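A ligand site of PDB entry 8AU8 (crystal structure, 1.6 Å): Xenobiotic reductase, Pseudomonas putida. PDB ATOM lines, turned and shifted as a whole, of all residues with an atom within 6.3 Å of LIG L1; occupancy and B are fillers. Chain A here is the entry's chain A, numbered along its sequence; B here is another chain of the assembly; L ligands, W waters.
An oxygen (O2) of LIG L1 sits close to a nitrogen (N2) of LG2 L2 (3.3 Å).
A ring nitrogen (ND1) of His 181 is in hydrogen-bond range of an oxygen (O2) of LIG L1 (2.8 Å). A ring nitrogen (NE2) of His 178 sits at hydrogen-bond distance from an oxygen (O2) of LIG L1 (3.0 Å). NE2 of His 178 lies within hydrogen-bond range of O1 of LG2 L2 (3.3 Å). The backbone NH of Trp 302 is in hydrogen-bond range of an oxygen (O6) of LG2 L2, 3.1 Å away. N of Ala 57 is in hydrogen-bond range of O2 of LG2 L2. N of Cys 25 lies within hydrogen-bond range of N3 of LG2 L2 (2.8 Å). SG of Cys 25 lies within hydrogen-bond range of O2 of LG2 L2, at 3.2 Å. The side-chain amide oxygen of Gln 99 sits at hydrogen-bond distance from a nitrogen (N2) of LG2 L2, at 2.8 Å. An oxygen (O1) of LG2 L2 lies within hydrogen-bond range of the guanidinium group (NH1) of Arg 231. The backbone carbonyl oxygen of Pro 23 is in hydrogen-bond range of an oxygen (O3) of LG2 L2 (2.9 Å).
SG of Cys 25 touches C5 of LIG L1, 3.9 Å away. Tyr 27 touches LIG L1 (OH to N1, 3.9 Å). CB of Ala 57 touches C2 of LIG L1 (3.4 Å). Ile 66 touches LIG L1 (CD1 to C5, 3.5 Å). Tyr 183 touches LIG L1 (CE2 to O2, 3.3 Å). Phe 269 touches LIG L1 (CG to C4, 3.4 Å). CH2 of Trp 302 touches O3 of LIG L1 (3.3 Å).
Water W2 lies within hydrogen-bond range of OH of Tyr 27 and O4 of LIG L1. Water W1 lies within hydrogen-bond range of NZ of Lys 106 (2.6 Å), O of His 181 (3.0 Å), OH of Tyr 183 (3.2 Å) and O1 of LIG L1 (3.4 Å).
O of His 181 is in hydrogen-bond range of NZ of Lys 106, 3.0 Å away. N of Ala 180 lies within hydrogen-bond range of ND1 of His 178, 3.3 Å away. The backbone NH (N) of Ala 57 lies close to the side-chain amide oxygen (OE1) of Gln 99, 3.5 Å away. The side-chain amino group of Lys 106 is in hydrogen-bond range of the backbone carbonyl oxygen of Phe 269, 2.8 Å away.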
ATOM      1  N   PRO A  23       0.261  22.327  25.564  1.00  0.00           N
ATOM      2  CA  PRO A  23      -1.166  22.527  25.286  1.00  0.00           C
ATOM      3  C   PRO A  23      -1.930  22.872  26.553  1.00  0.00           C
ATOM      4  O   PRO A  23      -1.788  22.202  27.589  1.00  0.00           O
ATOM      5  CB  PRO A  23      -1.604  21.182  24.695  1.00  0.00           C
ATOM      6  CG  PRO A  23      -0.569  20.190  25.217  1.00  0.00           C
ATOM      7  CD  PRO A  23       0.715  20.958  25.274  1.00  0.00           C
ATOM      8  N   CYS A  25      -5.930  23.804  27.328  1.00  0.00           N
ATOM      9  CA  CYS A  25      -7.335  24.034  27.045  1.00  0.00           C
ATOM     10  C   CYS A  25      -7.804  25.364  27.610  1.00  0.00           C
ATOM     11  O   CYS A  25      -7.539  25.688  28.776  1.00  0.00           O
ATOM     12  CB  CYS A  25      -8.177  22.914  27.646  1.00  0.00           C
ATOM     13  SG  CYS A  25      -8.203  21.414  26.659  1.00  0.00           S
ATOM     14  N   TYR A  27     -11.294  26.292  26.959  1.00  0.00           N
ATOM     15  CA  TYR A  27     -12.726  26.087  27.192  1.00  0.00           C
ATOM     16  C   TYR A  27     -13.556  27.286  26.706  1.00  0.00           C
ATOM     17  O   TYR A  27     -14.594  27.608  27.269  1.00  0.00           O
ATOM     18  CB  TYR A  27     -13.006  25.784  28.670  1.00  0.00           C
ATOM     19  CG  TYR A  27     -12.120  24.703  29.258  1.00  0.00           C
ATOM     20  CD1 TYR A  27     -12.434  23.354  29.113  1.00  0.00           C
ATOM     21  CD2 TYR A  27     -10.938  25.026  29.940  1.00  0.00           C
ATOM     22  CE1 TYR A  27     -11.610  22.357  29.642  1.00  0.00           C
ATOM     23  CE2 TYR A  27     -10.110  24.030  30.478  1.00  0.00           C
ATOM     24  CZ  TYR A  27     -10.465  22.702  30.323  1.00  0.00           C
ATOM     25  OH  TYR A  27      -9.655  21.714  30.838  1.00  0.00           O
ATOM     26  N   ALA A  57      -5.426  20.884  23.439  1.00  0.00           N
ATOM     27  CA  ALA A  57      -6.119  19.662  23.023  1.00  0.00           C
ATOM     28  C   ALA A  57      -7.297  19.991  22.132  1.00  0.00           C
ATOM     29  O   ALA A  57      -8.254  20.648  22.555  1.00  0.00           O
ATOM     30  CB  ALA A  57      -6.609  18.901  24.240  1.00  0.00           C
ATOM     31  N   ILE A  66     -13.542  17.417  25.740  1.00  0.00           N
ATOM     32  CA  ILE A  66     -13.818  17.285  27.161  1.00  0.00           C
ATOM     33  C   ILE A  66     -15.143  17.956  27.502  1.00  0.00           C
ATOM     34  O   ILE A  66     -16.008  17.355  28.133  1.00  0.00           O
ATOM     35  CB  ILE A  66     -12.674  17.856  28.002  1.00  0.00           C
ATOM     36  CG1 ILE A  66     -11.354  17.212  27.614  1.00  0.00           C
ATOM     37  CG2 ILE A  66     -12.973  17.661  29.500  1.00  0.00           C
ATOM     38  CD1 ILE A  66     -10.159  17.896  28.261  1.00  0.00           C
ATOM     39  N   GLN A  99      -1.946  19.912  19.558  1.00  0.00           N
ATOM     40  CA  GLN A  99      -2.240  18.631  20.188  1.00  0.00           C
ATOM     41  C   GLN A  99      -3.626  18.172  19.742  1.00  0.00           C
ATOM     42  O   GLN A  99      -4.611  18.872  19.978  1.00  0.00           O
ATOM     43  CB  GLN A  99      -2.199  18.761  21.713  1.00  0.00           C
ATOM     44  CG  GLN A  99      -2.307  17.400  22.415  1.00  0.00           C
ATOM     45  CD  GLN A  99      -2.550  17.532  23.900  1.00  0.00           C
ATOM     46  OE1 GLN A  99      -3.534  18.128  24.320  1.00  0.00           O
ATOM     47  NE2 GLN A  99      -1.643  16.952  24.704  1.00  0.00           N
ATOM     48  N   ALA A 101      -6.657  15.249  19.942  1.00  0.00           N
ATOM     49  CA  ALA A 101      -7.059  14.586  21.181  1.00  0.00           C
ATOM     50  C   ALA A 101      -8.413  13.915  21.046  1.00  0.00           C
ATOM     51  O   ALA A 101      -9.209  14.216  20.155  1.00  0.00           O
ATOM     52  CB  ALA A 101      -7.110  15.599  22.335  1.00  0.00           C
ATOM     53  N   LYS A 106     -13.472  10.600  29.953  1.00  0.00           N
ATOM     54  CA  LYS A 106     -13.506  11.875  30.654  1.00  0.00           C
ATOM     55  C   LYS A 106     -14.257  12.957  29.869  1.00  0.00           C
ATOM     56  O   LYS A 106     -14.331  14.102  30.314  1.00  0.00           O
ATOM     57  CB  LYS A 106     -12.064  12.333  30.955  1.00  0.00           C
ATOM     58  CG  LYS A 106     -11.272  11.355  31.828  1.00  0.00           C
ATOM     59  CD  LYS A 106     -10.037  12.076  32.387  1.00  0.00           C
ATOM     60  CE  LYS A 106      -9.301  11.244  33.422  1.00  0.00           C
ATOM     61  NZ  LYS A 106      -8.100  11.983  33.942  1.00  0.00           N
ATOM     62  N   HIS A 178      -2.376  13.143  21.643  1.00  0.00           N
ATOM     63  CA  HIS A 178      -2.658  13.206  23.084  1.00  0.00           C
ATOM     64  C   HIS A 178      -2.941  11.807  23.616  1.00  0.00           C
ATOM     65  O   HIS A 178      -4.085  11.369  23.692  1.00  0.00           O
ATOM     66  CB  HIS A 178      -3.821  14.136  23.392  1.00  0.00           C
ATOM     67  CG  HIS A 178      -3.900  14.498  24.831  1.00  0.00           C
ATOM     68  ND1 HIS A 178      -3.102  13.911  25.791  1.00  0.00           N
ATOM     69  CD2 HIS A 178      -4.634  15.430  25.491  1.00  0.00           C
ATOM     70  CE1 HIS A 178      -3.362  14.439  26.971  1.00  0.00           C
ATOM     71  NE2 HIS A 178      -4.286  15.372  26.822  1.00  0.00           N
ATOM     72  N   ALA A 180      -2.154  10.885  26.754  1.00  0.00           N
ATOM     73  CA  ALA A 180      -1.863  11.004  28.187  1.00  0.00           C
ATOM     74  C   ALA A 180      -3.113  11.392  28.970  1.00  0.00           C
ATOM     75  O   ALA A 180      -4.202  11.555  28.410  1.00  0.00           O
ATOM     76  CB  ALA A 180      -0.739  12.023  28.411  1.00  0.00           C
ATOM     77  N   HIS A 181      -2.958  11.497  30.289  1.00  0.00           N
ATOM     78  CA  HIS A 181      -3.904  12.166  31.172  1.00  0.00           C
ATOM     79  C   HIS A 181      -5.258  11.481  31.253  1.00  0.00           C
ATOM     80  O   HIS A 181      -6.272  12.125  31.583  1.00  0.00           O
ATOM     81  CB  HIS A 181      -4.041  13.645  30.769  1.00  0.00           C
ATOM     82  CG  HIS A 181      -2.750  14.413  30.834  1.00  0.00           C
ATOM     83  ND1 HIS A 181      -2.612  15.694  30.354  1.00  0.00           N
ATOM     84  CD2 HIS A 181      -1.544  14.063  31.336  1.00  0.00           C
ATOM     85  CE1 HIS A 181      -1.362  16.100  30.545  1.00  0.00           C
ATOM     86  NE2 HIS A 181      -0.707  15.134  31.148  1.00  0.00           N
ATOM     87  N   TYR A 183      -7.252  10.146  29.051  1.00  0.00           N
ATOM     88  CA  TYR A 183      -8.181  10.251  27.933  1.00  0.00           C
ATOM     89  C   TYR A 183      -8.074   8.970  27.090  1.00  0.00           C
ATOM     90  O   TYR A 183      -7.541   7.950  27.535  1.00  0.00           O
ATOM     91  CB  TYR A 183      -7.887  11.532  27.172  1.00  0.00           C
ATOM     92  CG  TYR A 183      -8.003  12.747  28.072  1.00  0.00           C
ATOM     93  CD1 TYR A 183      -9.217  13.070  28.679  1.00  0.00           C
ATOM     94  CD2 TYR A 183      -6.906  13.560  28.335  1.00  0.00           C
ATOM     95  CE1 TYR A 183      -9.331  14.188  29.522  1.00  0.00           C
ATOM     96  CE2 TYR A 183      -7.018  14.682  29.164  1.00  0.00           C
ATOM     97  CZ  TYR A 183      -8.231  14.985  29.759  1.00  0.00           C
ATOM     98  OH  TYR A 183      -8.329  16.098  30.604  1.00  0.00           O
ATOM     99  N   ARG A 231       2.151  12.971  23.605  1.00  0.00           N
ATOM    100  CA  ARG A 231       2.197  13.062  25.057  1.00  0.00           C
ATOM    101  C   ARG A 231       1.684  11.754  25.628  1.00  0.00           C
ATOM    102  O   ARG A 231       0.697  11.182  25.152  1.00  0.00           O
ATOM    103  CB  ARG A 231       1.341  14.238  25.559  1.00  0.00           C
ATOM    104  CG  ARG A 231       1.680  14.649  26.984  1.00  0.00           C
ATOM    105  CD  ARG A 231       1.122  16.031  27.319  1.00  0.00           C
ATOM    106  NE  ARG A 231       1.908  16.641  28.393  1.00  0.00           N
ATOM    107  CZ  ARG A 231       1.636  17.825  28.931  1.00  0.00           C
ATOM    108  NH1 ARG A 231       0.544  18.499  28.615  1.00  0.00           N
ATOM    109  NH2 ARG A 231       2.483  18.337  29.826  1.00  0.00           N
ATOM    110  N   VAL A 267       2.102  12.256  33.479  1.00  0.00           N
ATOM    111  CA  VAL A 267       1.495  11.315  34.409  1.00  0.00           C
ATOM    112  C   VAL A 267       0.225  10.787  33.769  1.00  0.00           C
ATOM    113  O   VAL A 267      -0.392  11.452  32.938  1.00  0.00           O
ATOM    114  CB  VAL A 267       1.237  12.004  35.772  1.00  0.00           C
ATOM    115  CG1 VAL A 267       0.435  11.139  36.708  1.00  0.00           C
ATOM    116  CG2 VAL A 267       2.559  12.420  36.418  1.00  0.00           C
ATOM    117  N   PHE A 269      -2.872   9.868  35.068  1.00  0.00           N
ATOM    118  CA  PHE A 269      -4.187  10.333  35.520  1.00  0.00           C
ATOM    119  C   PHE A 269      -5.322   9.414  35.059  1.00  0.00           C
ATOM    120  O   PHE A 269      -6.430   9.877  34.775  1.00  0.00           O
ATOM    121  CB  PHE A 269      -4.455  11.771  35.049  1.00  0.00           C
ATOM    122  CG  PHE A 269      -3.467  12.774  35.555  1.00  0.00           C
ATOM    123  CD1 PHE A 269      -3.511  13.221  36.872  1.00  0.00           C
ATOM    124  CD2 PHE A 269      -2.493  13.296  34.712  1.00  0.00           C
ATOM    125  CE1 PHE A 269      -2.590  14.145  37.341  1.00  0.00           C
ATOM    126  CE2 PHE A 269      -1.581  14.230  35.175  1.00  0.00           C
ATOM    127  CZ  PHE A 269      -1.623  14.644  36.492  1.00  0.00           C
ATOM    128  N   TRP A 302       4.844  20.484  34.735  1.00  0.00           N
ATOM    129  CA  TRP A 302       4.316  20.262  36.086  1.00  0.00           C
ATOM    130  C   TRP A 302       5.322  20.737  37.117  1.00  0.00           C
ATOM    131  O   TRP A 302       5.799  19.953  37.950  1.00  0.00           O
ATOM    132  CB  TRP A 302       3.928  18.791  36.343  1.00  0.00           C
ATOM    133  CG  TRP A 302       2.979  18.163  35.317  1.00  0.00           C
ATOM    134  CD1 TRP A 302       3.306  17.276  34.311  1.00  0.00           C
ATOM    135  CD2 TRP A 302       1.555  18.367  35.216  1.00  0.00           C
ATOM    136  NE1 TRP A 302       2.171  16.919  33.600  1.00  0.00           N
ATOM    137  CE2 TRP A 302       1.091  17.584  34.128  1.00  0.00           C
ATOM    138  CE3 TRP A 302       0.635  19.135  35.933  1.00  0.00           C
ATOM    139  CZ2 TRP A 302      -0.253  17.561  33.756  1.00  0.00           C
ATOM    140  CZ3 TRP A 302      -0.693  19.107  35.563  1.00  0.00           C
ATOM    141  CH2 TRP A 302      -1.124  18.312  34.478  1.00  0.00           C
ATOM    142  N   TRP B 358      -7.059  28.808  37.221  1.00  0.00           N
ATOM    143  CA  TRP B 358      -5.869  28.003  37.429  1.00  0.00           C
ATOM    144  C   TRP B 358      -4.833  28.694  38.300  1.00  0.00           C
ATOM    145  O   TRP B 358      -4.074  28.031  39.001  1.00  0.00           O
ATOM    146  CB  TRP B 358      -5.254  27.648  36.068  1.00  0.00           C
ATOM    147  CG  TRP B 358      -6.311  27.114  35.169  1.00  0.00           C
ATOM    148  CD1 TRP B 358      -6.913  27.767  34.125  1.00  0.00           C
ATOM    149  CD2 TRP B 358      -6.952  25.843  35.272  1.00  0.00           C
ATOM    150  NE1 TRP B 358      -7.869  26.963  33.565  1.00  0.00           N
ATOM    151  CE2 TRP B 358      -7.924  25.780  34.250  1.00  0.00           C
ATOM    152  CE3 TRP B 358      -6.812  24.756  36.136  1.00  0.00           C
ATOM    153  CZ2 TRP B 358      -8.726  24.657  34.057  1.00  0.00           C
ATOM    154  CZ3 TRP B 358      -7.609  23.645  35.940  1.00  0.00           C
ATOM    155  CH2 TRP B 358      -8.555  23.602  34.911  1.00  0.00           C
HETATM  156  N1  LIG L   1      -6.467  19.485  31.394  1.00  0.00           N
HETATM  157  C1  LIG L   1      -4.633  17.793  32.030  1.00  0.00           C
HETATM  158  C2  LIG L   1      -6.689  17.630  27.388  1.00  0.00           C
HETATM  159  C3  LIG L   1      -4.283  16.254  33.768  1.00  0.00           C
HETATM  160  C4  LIG L   1      -5.207  15.610  34.798  1.00  0.00           C
HETATM  161  C5  LIG L   1      -6.707  18.393  28.698  1.00  0.00           C
HETATM  162  C6  LIG L   1      -5.602  17.879  29.609  1.00  0.00           C
HETATM  163  C7  LIG L   1      -5.572  18.418  31.017  1.00  0.00           C
HETATM  164  O1  LIG L   1      -5.069  16.634  32.677  1.00  0.00           O
HETATM  165  O2  LIG L   1      -4.806  17.090  29.226  1.00  0.00           O
HETATM  166  O3  LIG L   1      -3.561  18.262  32.263  1.00  0.00           O
HETATM  167  O4  LIG L   1      -6.248  19.796  32.747  1.00  0.00           O
HETATM  168  N1  LG2 L   2      -2.337  19.121  29.049  1.00  0.00           N
HETATM  169  C1  LG2 L   2      -2.531  18.556  27.798  1.00  0.00           C
HETATM  170  O1  LG2 L   2      -1.850  17.574  27.463  1.00  0.00           O
HETATM  171  N2  LG2 L   2      -3.480  19.089  26.940  1.00  0.00           N
HETATM  172  C2  LG2 L   2      -4.250  20.176  27.306  1.00  0.00           C
HETATM  173  O2  LG2 L   2      -5.074  20.665  26.510  1.00  0.00           O
HETATM  174  C3  LG2 L   2      -4.063  20.725  28.574  1.00  0.00           C
HETATM  175  N3  LG2 L   2      -4.807  21.804  28.971  1.00  0.00           N
HETATM  176  C4  LG2 L   2      -4.494  22.441  30.141  1.00  0.00           C
HETATM  177  C5  LG2 L   2      -5.154  23.629  30.430  1.00  0.00           C
HETATM  178  C6  LG2 L   2      -4.850  24.353  31.565  1.00  0.00           C
HETATM  179  C7  LG2 L   2      -5.580  25.642  31.813  1.00  0.00           C
HETATM  180  C8  LG2 L   2      -3.867  23.862  32.424  1.00  0.00           C
HETATM  181  C9  LG2 L   2      -3.509  24.628  33.666  1.00  0.00           C
HETATM  182  C10 LG2 L   2      -3.204  22.665  32.133  1.00  0.00           C
HETATM  183  C11 LG2 L   2      -3.519  21.940  30.981  1.00  0.00           C
HETATM  184  N4  LG2 L   2      -2.858  20.755  30.678  1.00  0.00           N
HETATM  185  C12 LG2 L   2      -3.087  20.199  29.438  1.00  0.00           C
HETATM  186  C13 LG2 L   2      -1.519  20.454  31.330  1.00  0.00           C
HETATM  187  C14 LG2 L   2      -0.386  21.420  30.928  1.00  0.00           C
HETATM  188  O3  LG2 L   2       0.009  21.182  29.599  1.00  0.00           O
HETATM  189  C15 LG2 L   2       0.844  21.290  31.812  1.00  0.00           C
HETATM  190  O4  LG2 L   2       1.298  19.952  31.844  1.00  0.00           O
HETATM  191  C16 LG2 L   2       0.542  21.764  33.238  1.00  0.00           C
HETATM  192  O5  LG2 L   2       0.022  23.071  33.203  1.00  0.00           O
HETATM  193  C17 LG2 L   2       1.778  21.707  34.139  1.00  0.00           C
HETATM  194  O6  LG2 L   2       2.788  22.602  33.737  1.00  0.00           O
HETATM  195  P1  LG2 L   2       2.982  23.994  34.546  1.00  0.00           P
HETATM  196  O7  LG2 L   2       4.087  24.736  33.847  1.00  0.00           O
HETATM  197  O8  LG2 L   2       1.671  24.732  34.516  1.00  0.00           O
HETATM  198  O9  LG2 L   2       3.384  23.661  35.972  1.00  0.00           O
HETATM  199  O   HOH W   1      -7.551  14.342  33.124  1.00  0.00           O
HETATM  200  O   HOH W   2      -7.647  22.014  32.462  1.00  0.00           O
